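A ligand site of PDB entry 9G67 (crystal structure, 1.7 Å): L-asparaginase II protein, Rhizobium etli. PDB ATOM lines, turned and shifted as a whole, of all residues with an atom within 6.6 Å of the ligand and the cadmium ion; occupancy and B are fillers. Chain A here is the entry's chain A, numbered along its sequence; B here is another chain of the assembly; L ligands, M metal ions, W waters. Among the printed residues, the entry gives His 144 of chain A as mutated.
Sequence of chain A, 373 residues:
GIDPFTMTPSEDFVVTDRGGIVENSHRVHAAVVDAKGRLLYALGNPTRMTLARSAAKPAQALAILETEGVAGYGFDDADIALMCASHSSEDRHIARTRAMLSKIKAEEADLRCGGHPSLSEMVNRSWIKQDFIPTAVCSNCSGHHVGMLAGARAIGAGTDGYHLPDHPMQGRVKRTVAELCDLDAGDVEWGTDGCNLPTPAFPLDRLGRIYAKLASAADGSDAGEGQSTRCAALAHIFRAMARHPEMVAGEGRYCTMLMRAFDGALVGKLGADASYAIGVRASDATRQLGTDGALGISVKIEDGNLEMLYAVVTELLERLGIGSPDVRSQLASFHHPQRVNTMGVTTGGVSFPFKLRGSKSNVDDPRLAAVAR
The side-chain sulfur (SG) of Cys 195 binds the cadmium ion (2.6 Å).
The cadmium ion is bound by N1 of the ligand, at 2.6 Å.
SG of Cys 141 binds the cadmium ion, at 2.6 Å.
The cadmium ion has three donor atoms within binding distance.
Slightly farther from the cadmium ion lies O1 of the ligand (2.6 Å).
Slightly farther from the cadmium ion lies NZ of Lys 57 (2.7 Å).
Asp 193 touches the cadmium ion (OD2 to CD, 3.2 Å).
Along chain A the residues within 4 Å of the cadmium ion span positions 57 to 195.
The nearest printed residue that does not touch the cadmium ion is Ser 54 (4.1 Å).
O of Cys 195 lies close to NE2 of His 145.
The side-chain hydroxyl of Ser 139 sits close to the backbone NH of Cys 141 (3.0 Å).
The side-chain amino group (NZ) of Lys 57 lies within salt-bridge range of the side-chain carboxylate (OD2) of Asp 193.
The side-chain carboxylate of Asp 193 is in hydrogen-bond range of the side-chain hydroxyl of Thr 199.
The guanidinium group (NH1) of Arg 53 is in salt-bridge range of the side-chain carboxylate (OD2) of Asp 273 (2.8 Å).
The side-chain hydroxyl (OG) of Ser 86 is in hydrogen-bond range of the side-chain amino group (NZ) of Lys 269 (2.7 Å).
The guanidinium group (NH1) of Arg 253 sits at hydrogen-bond distance from the backbone carbonyl oxygen (O) of Ser 86 (2.9 Å).
The side-chain hydroxyl (OG1) of Thr 342 of chain B sits at hydrogen-bond distance from the backbone carbonyl oxygen (O) of Gly 194 (2.9 Å).
N of Cys 195 sits at hydrogen-bond distance from O1 of the ligand (3.0 Å).
The backbone NH (N) of Ser 54 is in hydrogen-bond range of an oxygen (O2) of the ligand (2.8 Å).
An oxygen (O2) of the ligand lies close to the side-chain hydroxyl of Ser 54 (3.0 Å).
OD2 of Asp 193 sits close to N1 of the ligand (2.8 Å).
NH2 of Arg 53 is in salt-bridge range of O3 of the ligand (2.8 Å).
OG of Ser 86 sits at hydrogen-bond distance from N2 of the ligand (2.9 Å).
N of Ala 272 sits at hydrogen-bond distance from O2 of the ligand (2.9 Å).
N of Gly 194 sits at hydrogen-bond distance from O3 of the ligand (3.1 Å).
Water W1 lies within hydrogen-bond range of an oxygen (O1) of the ligand (2.9 Å), the side-chain amide nitrogen of Asn 140 (3.2 Å) and the backbone NH of Cys 195 (3.5 Å).
OD1 of Asn 140 touches C3 of the ligand (3.8 Å).
C of Gly 271 touches O2 of the ligand, at 3.9 Å.
Hydrophobic or aromatic side chains within 4 Å of the ligand: Ala 272.
Of the 28 residues printed, 11 come within 4 Å of the ligand.
The nearest printed residue that does not touch the ligand is Leu 270 (4.4 Å).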
ATOM      1  N   ALA A  52      -7.677   4.713 -16.383  1.00  0.00           N
ATOM      2  CA  ALA A  52      -6.884   3.514 -16.191  1.00  0.00           C
ATOM      3  C   ALA A  52      -7.560   2.522 -15.266  1.00  0.00           C
ATOM      4  O   ALA A  52      -7.253   1.322 -15.331  1.00  0.00           O
ATOM      5  CB  ALA A  52      -5.498   3.870 -15.629  1.00  0.00           C
ATOM      6  N   ARG A  53      -8.456   2.999 -14.387  1.00  0.00           N
ATOM      7  CA  ARG A  53      -9.194   2.150 -13.483  1.00  0.00           C
ATOM      8  C   ARG A  53      -8.177   1.282 -12.732  1.00  0.00           C
ATOM      9  O   ARG A  53      -7.132   1.808 -12.333  1.00  0.00           O
ATOM     10  CB  ARG A  53     -10.236   1.341 -14.261  1.00  0.00           C
ATOM     11  CG  ARG A  53     -11.173   2.255 -15.076  1.00  0.00           C
ATOM     12  CD  ARG A  53     -12.053   3.150 -14.178  1.00  0.00           C
ATOM     13  NE  ARG A  53     -13.037   2.369 -13.421  1.00  0.00           N
ATOM     14  CZ  ARG A  53     -14.092   1.730 -13.918  1.00  0.00           C
ATOM     15  NH1 ARG A  53     -14.414   1.787 -15.199  1.00  0.00           N
ATOM     16  NH2 ARG A  53     -14.846   0.990 -13.095  1.00  0.00           N
ATOM     17  N   SER A  54      -8.439  -0.009 -12.536  1.00  0.00           N
ATOM     18  CA  SER A  54      -7.478  -0.785 -11.747  1.00  0.00           C
ATOM     19  C   SER A  54      -6.151  -1.051 -12.441  1.00  0.00           C
ATOM     20  O   SER A  54      -5.254  -1.588 -11.786  1.00  0.00           O
ATOM     21  CB  SER A  54      -8.054  -2.110 -11.322  1.00  0.00           C
ATOM     22  OG  SER A  54      -9.000  -1.889 -10.292  1.00  0.00           O
ATOM     23  N   ALA A  55      -5.990  -0.714 -13.732  1.00  0.00           N
ATOM     24  CA  ALA A  55      -4.630  -0.803 -14.252  1.00  0.00           C
ATOM     25  C   ALA A  55      -3.720   0.235 -13.605  1.00  0.00           C
ATOM     26  O   ALA A  55      -2.489   0.093 -13.694  1.00  0.00           O
ATOM     27  CB  ALA A  55      -4.597  -0.650 -15.777  1.00  0.00           C
ATOM     28  N   LYS A  57      -3.789   0.540 -10.251  1.00  0.00           N
ATOM     29  CA  LYS A  57      -3.532   0.042  -8.894  1.00  0.00           C
ATOM     30  C   LYS A  57      -2.056  -0.092  -8.541  1.00  0.00           C
ATOM     31  O   LYS A  57      -1.669   0.330  -7.441  1.00  0.00           O
ATOM     32  CB  LYS A  57      -4.237  -1.296  -8.673  1.00  0.00           C
ATOM     33  CG  LYS A  57      -5.373  -1.311  -7.701  1.00  0.00           C
ATOM     34  CD  LYS A  57      -6.285  -0.137  -7.912  1.00  0.00           C
ATOM     35  CE  LYS A  57      -7.645  -0.370  -7.216  1.00  0.00           C
ATOM     36  NZ  LYS A  57      -8.484   0.861  -7.348  1.00  0.00           N
ATOM     37  N   GLN A  60      -0.779   3.395  -7.728  1.00  0.00           N
ATOM     38  CA  GLN A  60      -1.347   3.860  -6.468  1.00  0.00           C
ATOM     39  C   GLN A  60      -0.734   3.122  -5.299  1.00  0.00           C
ATOM     40  O   GLN A  60      -0.500   3.725  -4.241  1.00  0.00           O
ATOM     41  CB  GLN A  60      -2.870   3.696  -6.498  1.00  0.00           C
ATOM     42  CG  GLN A  60      -3.548   4.524  -7.595  1.00  0.00           C
ATOM     43  CD  GLN A  60      -5.061   4.385  -7.641  1.00  0.00           C
ATOM     44  OE1 GLN A  60      -5.708   4.977  -8.495  1.00  0.00           O
ATOM     45  NE2 GLN A  60      -5.624   3.596  -6.733  1.00  0.00           N
ATOM     46  N   ALA A  85      -4.418  -5.559  -6.921  1.00  0.00           N
ATOM     47  CA  ALA A  85      -5.282  -6.549  -7.523  1.00  0.00           C
ATOM     48  C   ALA A  85      -6.659  -5.996  -7.899  1.00  0.00           C
ATOM     49  O   ALA A  85      -7.092  -4.954  -7.405  1.00  0.00           O
ATOM     50  CB  ALA A  85      -5.470  -7.756  -6.585  1.00  0.00           C
ATOM     51  N   SER A  86      -7.304  -6.702  -8.855  1.00  0.00           N
ATOM     52  CA  SER A  86      -8.767  -6.792  -9.070  1.00  0.00           C
ATOM     53  C   SER A  86      -9.080  -8.279  -8.933  1.00  0.00           C
ATOM     54  O   SER A  86      -9.259  -9.004  -9.917  1.00  0.00           O
ATOM     55  CB  SER A  86      -9.230  -6.266 -10.469  1.00  0.00           C
ATOM     56  OG  SER A  86      -8.670  -4.985 -10.732  1.00  0.00           O
ATOM     57  N   LEU A 119     -16.026 -10.818 -10.063  1.00  0.00           N
ATOM     58  CA  LEU A 119     -15.430 -10.824 -11.400  1.00  0.00           C
ATOM     59  C   LEU A 119     -15.348 -12.221 -11.996  1.00  0.00           C
ATOM     60  O   LEU A 119     -15.267 -12.351 -13.225  1.00  0.00           O
ATOM     61  CB  LEU A 119     -14.037 -10.185 -11.340  1.00  0.00           C
ATOM     62  CG  LEU A 119     -14.056  -8.725 -10.855  1.00  0.00           C
ATOM     63  CD1 LEU A 119     -12.682  -8.123 -10.998  1.00  0.00           C
ATOM     64  CD2 LEU A 119     -15.054  -7.964 -11.685  1.00  0.00           C
ATOM     65  N   SER A 139     -14.840  -6.837  -1.934  1.00  0.00           N
ATOM     66  CA  SER A 139     -14.533  -5.957  -3.059  1.00  0.00           C
ATOM     67  C   SER A 139     -13.247  -6.395  -3.733  1.00  0.00           C
ATOM     68  O   SER A 139     -12.270  -6.763  -3.083  1.00  0.00           O
ATOM     69  CB  SER A 139     -14.423  -4.499  -2.586  1.00  0.00           C
ATOM     70  OG  SER A 139     -13.530  -3.738  -3.385  1.00  0.00           O
ATOM     71  N   ASN A 140     -13.272  -6.383  -5.071  1.00  0.00           N
ATOM     72  CA  ASN A 140     -12.104  -6.785  -5.836  1.00  0.00           C
ATOM     73  C   ASN A 140     -10.911  -5.881  -5.541  1.00  0.00           C
ATOM     74  O   ASN A 140      -9.759  -6.263  -5.819  1.00  0.00           O
ATOM     75  CB  ASN A 140     -12.443  -6.766  -7.334  1.00  0.00           C
ATOM     76  CG  ASN A 140     -12.467  -5.350  -7.908  1.00  0.00           C
ATOM     77  OD1 ASN A 140     -11.472  -4.885  -8.481  1.00  0.00           O
ATOM     78  ND2 ASN A 140     -13.579  -4.648  -7.747  1.00  0.00           N
ATOM     79  N   CYS A 141     -11.156  -4.704  -4.963  1.00  0.00           N
ATOM     80  CA  CYS A 141     -10.137  -3.751  -4.582  1.00  0.00           C
ATOM     81  C   CYS A 141      -9.894  -3.720  -3.072  1.00  0.00           C
ATOM     82  O   CYS A 141      -9.256  -2.797  -2.584  1.00  0.00           O
ATOM     83  CB  CYS A 141     -10.515  -2.360  -5.074  1.00  0.00           C
ATOM     84  SG  CYS A 141     -11.025  -2.314  -6.817  1.00  0.00           S
ATOM     85  N   HIS A 144      -6.279  -3.176  -1.890  1.00  0.00           N
ATOM     86  CA  HIS A 144      -5.863  -1.797  -2.097  1.00  0.00           C
ATOM     87  C   HIS A 144      -6.388  -0.882  -0.997  1.00  0.00           C
ATOM     88  O   HIS A 144      -5.640  -0.047  -0.450  1.00  0.00           O
ATOM     89  CB  HIS A 144      -6.354  -1.342  -3.456  1.00  0.00           C
ATOM     90  CG  HIS A 144      -5.794  -0.018  -3.862  1.00  0.00           C
ATOM     91  ND1 HIS A 144      -4.501   0.116  -4.326  1.00  0.00           N
ATOM     92  CD2 HIS A 144      -6.339   1.212  -3.837  1.00  0.00           C
ATOM     93  CE1 HIS A 144      -4.280   1.393  -4.594  1.00  0.00           C
ATOM     94  NE2 HIS A 144      -5.363   2.080  -4.294  1.00  0.00           N
ATOM     95  N   HIS A 145      -7.661  -1.029  -0.643  1.00  0.00           N
ATOM     96  CA  HIS A 145      -8.243  -0.253   0.440  1.00  0.00           C
ATOM     97  C   HIS A 145      -7.554  -0.517   1.770  1.00  0.00           C
ATOM     98  O   HIS A 145      -7.447   0.383   2.619  1.00  0.00           O
ATOM     99  CB  HIS A 145      -9.720  -0.554   0.565  1.00  0.00           C
ATOM    100  CG  HIS A 145     -10.541   0.198  -0.412  1.00  0.00           C
ATOM    101  ND1 HIS A 145     -11.303   1.291  -0.050  1.00  0.00           N
ATOM    102  CD2 HIS A 145     -10.666   0.076  -1.753  1.00  0.00           C
ATOM    103  CE1 HIS A 145     -11.898   1.779  -1.129  1.00  0.00           C
ATOM    104  NE2 HIS A 145     -11.534   1.055  -2.171  1.00  0.00           N
ATOM    105  N   ASP A 193     -14.150   5.995  -8.642  1.00  0.00           N
ATOM    106  CA  ASP A 193     -14.151   4.582  -9.072  1.00  0.00           C
ATOM    107  C   ASP A 193     -15.351   3.814  -8.523  1.00  0.00           C
ATOM    108  O   ASP A 193     -16.077   4.286  -7.655  1.00  0.00           O
ATOM    109  CB  ASP A 193     -12.864   3.899  -8.596  1.00  0.00           C
ATOM    110  CG  ASP A 193     -12.203   3.084  -9.703  1.00  0.00           C
ATOM    111  OD1 ASP A 193     -12.895   2.808 -10.725  1.00  0.00           O
ATOM    112  OD2 ASP A 193     -10.991   2.728  -9.540  1.00  0.00           O
ATOM    113  N   GLY A 194     -15.548   2.585  -9.039  1.00  0.00           N
ATOM    114  CA  GLY A 194     -16.611   1.740  -8.492  1.00  0.00           C
ATOM    115  C   GLY A 194     -16.419   1.446  -7.011  1.00  0.00           C
ATOM    116  O   GLY A 194     -17.402   1.232  -6.270  1.00  0.00           O
ATOM    117  N   CYS A 195     -15.176   1.431  -6.556  1.00  0.00           N
ATOM    118  CA  CYS A 195     -14.853   1.159  -5.162  1.00  0.00           C
ATOM    119  C   CYS A 195     -14.848   2.421  -4.309  1.00  0.00           C
ATOM    120  O   CYS A 195     -14.484   2.352  -3.141  1.00  0.00           O
ATOM    121  CB  CYS A 195     -13.503   0.449  -5.062  1.00  0.00           C
ATOM    122  SG  CYS A 195     -12.100   1.493  -5.555  1.00  0.00           S
ATOM    123  N   ASN A 196     -15.224   3.564  -4.881  1.00  0.00           N
ATOM    124  CA  ASN A 196     -15.456   4.832  -4.196  1.00  0.00           C
ATOM    125  C   ASN A 196     -14.181   5.617  -3.893  1.00  0.00           C
ATOM    126  O   ASN A 196     -14.235   6.625  -3.137  1.00  0.00           O
ATOM    127  CB  ASN A 196     -16.235   4.639  -2.898  1.00  0.00           C
ATOM    128  CG  ASN A 196     -17.033   5.854  -2.507  1.00  0.00           C
ATOM    129  OD1 ASN A 196     -17.488   6.603  -3.365  1.00  0.00           O
ATOM    130  ND2 ASN A 196     -17.216   6.055  -1.210  1.00  0.00           N
ATOM    131  N   LEU A 197     -13.006   5.211  -4.454  1.00  0.00           N
ATOM    132  CA  LEU A 197     -11.755   5.972  -4.413  1.00  0.00           C
ATOM    133  C   LEU A 197     -11.643   6.881  -5.627  1.00  0.00           C
ATOM    134  O   LEU A 197     -12.279   6.647  -6.658  1.00  0.00           O
ATOM    135  CB  LEU A 197     -10.581   5.012  -4.403  1.00  0.00           C
ATOM    136  CG  LEU A 197     -10.302   4.275  -3.108  1.00  0.00           C
ATOM    137  CD1 LEU A 197      -9.241   3.235  -3.363  1.00  0.00           C
ATOM    138  CD2 LEU A 197      -9.807   5.274  -2.062  1.00  0.00           C
ATOM    139  N   THR A 199      -9.950   8.039  -9.076  1.00  0.00           N
ATOM    140  CA  THR A 199      -9.368   7.164 -10.090  1.00  0.00           C
ATOM    141  C   THR A 199      -8.904   8.048 -11.251  1.00  0.00           C
ATOM    142  O   THR A 199      -9.627   9.000 -11.640  1.00  0.00           O
ATOM    143  CB  THR A 199     -10.382   6.066 -10.533  1.00  0.00           C
ATOM    144  OG1 THR A 199      -9.715   5.058 -11.277  1.00  0.00           O
ATOM    145  CG2 THR A 199     -11.563   6.622 -11.365  1.00  0.00           C
ATOM    146  N   ARG A 253      -8.388 -16.479 -14.487  1.00  0.00           N
ATOM    147  CA  ARG A 253      -8.409 -15.106 -14.933  1.00  0.00           C
ATOM    148  C   ARG A 253      -7.228 -14.830 -15.877  1.00  0.00           C
ATOM    149  O   ARG A 253      -6.132 -15.358 -15.686  1.00  0.00           O
ATOM    150  CB  ARG A 253      -8.358 -14.167 -13.723  1.00  0.00           C
ATOM    151  CG  ARG A 253      -9.568 -14.260 -12.807  1.00  0.00           C
ATOM    152  CD  ARG A 253     -10.704 -13.312 -13.300  1.00  0.00           C
ATOM    153  NE  ARG A 253     -10.253 -11.946 -13.542  1.00  0.00           N
ATOM    154  CZ  ARG A 253     -10.067 -11.033 -12.594  1.00  0.00           C
ATOM    155  NH1 ARG A 253     -10.263 -11.316 -11.316  1.00  0.00           N
ATOM    156  NH2 ARG A 253      -9.597  -9.826 -12.930  1.00  0.00           N
ATOM    157  N   LYS A 269      -2.019  -6.418 -16.063  1.00  0.00           N
ATOM    158  CA  LYS A 269      -3.054  -5.985 -15.131  1.00  0.00           C
ATOM    159  C   LYS A 269      -4.239  -5.448 -15.926  1.00  0.00           C
ATOM    160  O   LYS A 269      -4.043  -4.655 -16.844  1.00  0.00           O
ATOM    161  CB  LYS A 269      -2.513  -4.915 -14.158  1.00  0.00           C
ATOM    162  CG  LYS A 269      -3.529  -4.317 -13.206  1.00  0.00           C
ATOM    163  CD  LYS A 269      -3.882  -5.356 -12.122  1.00  0.00           C
ATOM    164  CE  LYS A 269      -5.124  -4.939 -11.336  1.00  0.00           C
ATOM    165  NZ  LYS A 269      -6.353  -5.454 -11.944  1.00  0.00           N
ATOM    166  N   LEU A 270      -5.444  -5.871 -15.549  1.00  0.00           N
ATOM    167  CA  LEU A 270      -6.694  -5.428 -16.164  1.00  0.00           C
ATOM    168  C   LEU A 270      -7.205  -4.120 -15.557  1.00  0.00           C
ATOM    169  O   LEU A 270      -7.115  -3.915 -14.341  1.00  0.00           O
ATOM    170  CB  LEU A 270      -7.772  -6.506 -15.991  1.00  0.00           C
ATOM    171  CG  LEU A 270      -9.203  -6.124 -16.285  1.00  0.00           C
ATOM    172  CD1 LEU A 270      -9.449  -6.206 -17.797  1.00  0.00           C
ATOM    173  CD2 LEU A 270     -10.122  -7.093 -15.531  1.00  0.00           C
ATOM    174  N   GLY A 271      -7.732  -3.247 -16.414  1.00  0.00           N
ATOM    175  CA  GLY A 271      -8.553  -2.126 -15.987  1.00  0.00           C
ATOM    176  C   GLY A 271      -9.993  -2.347 -16.422  1.00  0.00           C
ATOM    177  O   GLY A 271     -10.252  -2.700 -17.586  1.00  0.00           O
ATOM    178  N   ALA A 272     -10.927  -2.121 -15.491  1.00  0.00           N
ATOM    179  CA  ALA A 272     -12.341  -2.212 -15.835  1.00  0.00           C
ATOM    180  C   ALA A 272     -12.684  -1.332 -17.043  1.00  0.00           C
ATOM    181  O   ALA A 272     -12.044  -0.303 -17.313  1.00  0.00           O
ATOM    182  CB  ALA A 272     -13.196  -1.799 -14.637  1.00  0.00           C
ATOM    183  N   ASP A 273     -13.720  -1.778 -17.769  1.00  0.00           N
ATOM    184  CA  ASP A 273     -14.107  -1.209 -19.071  1.00  0.00           C
ATOM    185  C   ASP A 273     -12.999  -1.353 -20.117  1.00  0.00           C
ATOM    186  O   ASP A 273     -12.869  -0.534 -21.042  1.00  0.00           O
ATOM    187  CB  ASP A 273     -14.581   0.230 -18.914  1.00  0.00           C
ATOM    188  CG  ASP A 273     -15.949   0.289 -18.297  1.00  0.00           C
ATOM    189  OD1 ASP A 273     -16.854  -0.411 -18.831  1.00  0.00           O
ATOM    190  OD2 ASP A 273     -16.133   0.961 -17.273  1.00  0.00           O
ATOM    191  N   ARG B  18     -17.338   8.989 -16.816  1.00  0.00           N
ATOM    192  CA  ARG B  18     -17.108   8.953 -15.380  1.00  0.00           C
ATOM    193  C   ARG B  18     -16.668  10.355 -14.984  1.00  0.00           C
ATOM    194  O   ARG B  18     -15.598  10.801 -15.389  1.00  0.00           O
ATOM    195  CB  ARG B  18     -16.072   7.862 -15.047  1.00  0.00           C
ATOM    196  CG  ARG B  18     -15.854   7.590 -13.564  1.00  0.00           C
ATOM    197  CD  ARG B  18     -14.988   6.347 -13.376  1.00  0.00           C
ATOM    198  NE  ARG B  18     -15.680   5.186 -13.918  1.00  0.00           N
ATOM    199  CZ  ARG B  18     -16.461   4.381 -13.201  1.00  0.00           C
ATOM    200  NH1 ARG B  18     -16.623   4.547 -11.897  1.00  0.00           N
ATOM    201  NH2 ARG B  18     -17.107   3.393 -13.828  1.00  0.00           N
ATOM    202  N   THR B 342     -20.261   1.045  -5.791  1.00  0.00           N
ATOM    203  CA  THR B 342     -20.628   0.065  -4.760  1.00  0.00           C
ATOM    204  C   THR B 342     -21.024   0.707  -3.432  1.00  0.00           C
ATOM    205  O   THR B 342     -21.454  -0.019  -2.522  1.00  0.00           O
ATOM    206  CB  THR B 342     -19.476  -0.926  -4.541  1.00  0.00           C
ATOM    207  OG1 THR B 342     -18.337  -0.249  -3.990  1.00  0.00           O
ATOM    208  CG2 THR B 342     -19.076  -1.599  -5.880  1.00  0.00           C
HETATM  209  N1  LIG L   1     -11.071  -0.005 -10.068  1.00  0.00           N
HETATM  210  C1  LIG L   1     -12.291  -0.522 -10.675  1.00  0.00           C
HETATM  211  C2  LIG L   1     -13.508  -0.139  -9.851  1.00  0.00           C
HETATM  212  O1  LIG L   1     -13.486  -0.016  -8.623  1.00  0.00           O
HETATM  213  C3  LIG L   1     -12.210  -2.046 -10.844  1.00  0.00           C
HETATM  214  C4  LIG L   1     -11.227  -2.415 -11.937  1.00  0.00           C
HETATM  215  O2  LIG L   1     -10.762  -1.526 -12.657  1.00  0.00           O
HETATM  216  N2  LIG L   1     -10.894  -3.730 -12.070  1.00  0.00           N
HETATM  217  O3  LIG L   1     -14.530   0.069 -10.447  1.00  0.00           O
HETATM  218 CD    CD M   1     -11.100   0.202  -7.514  1.00  0.00          CD
HETATM  219  O   HOH W   1     -15.272  -1.968  -7.321  1.00  0.00           O
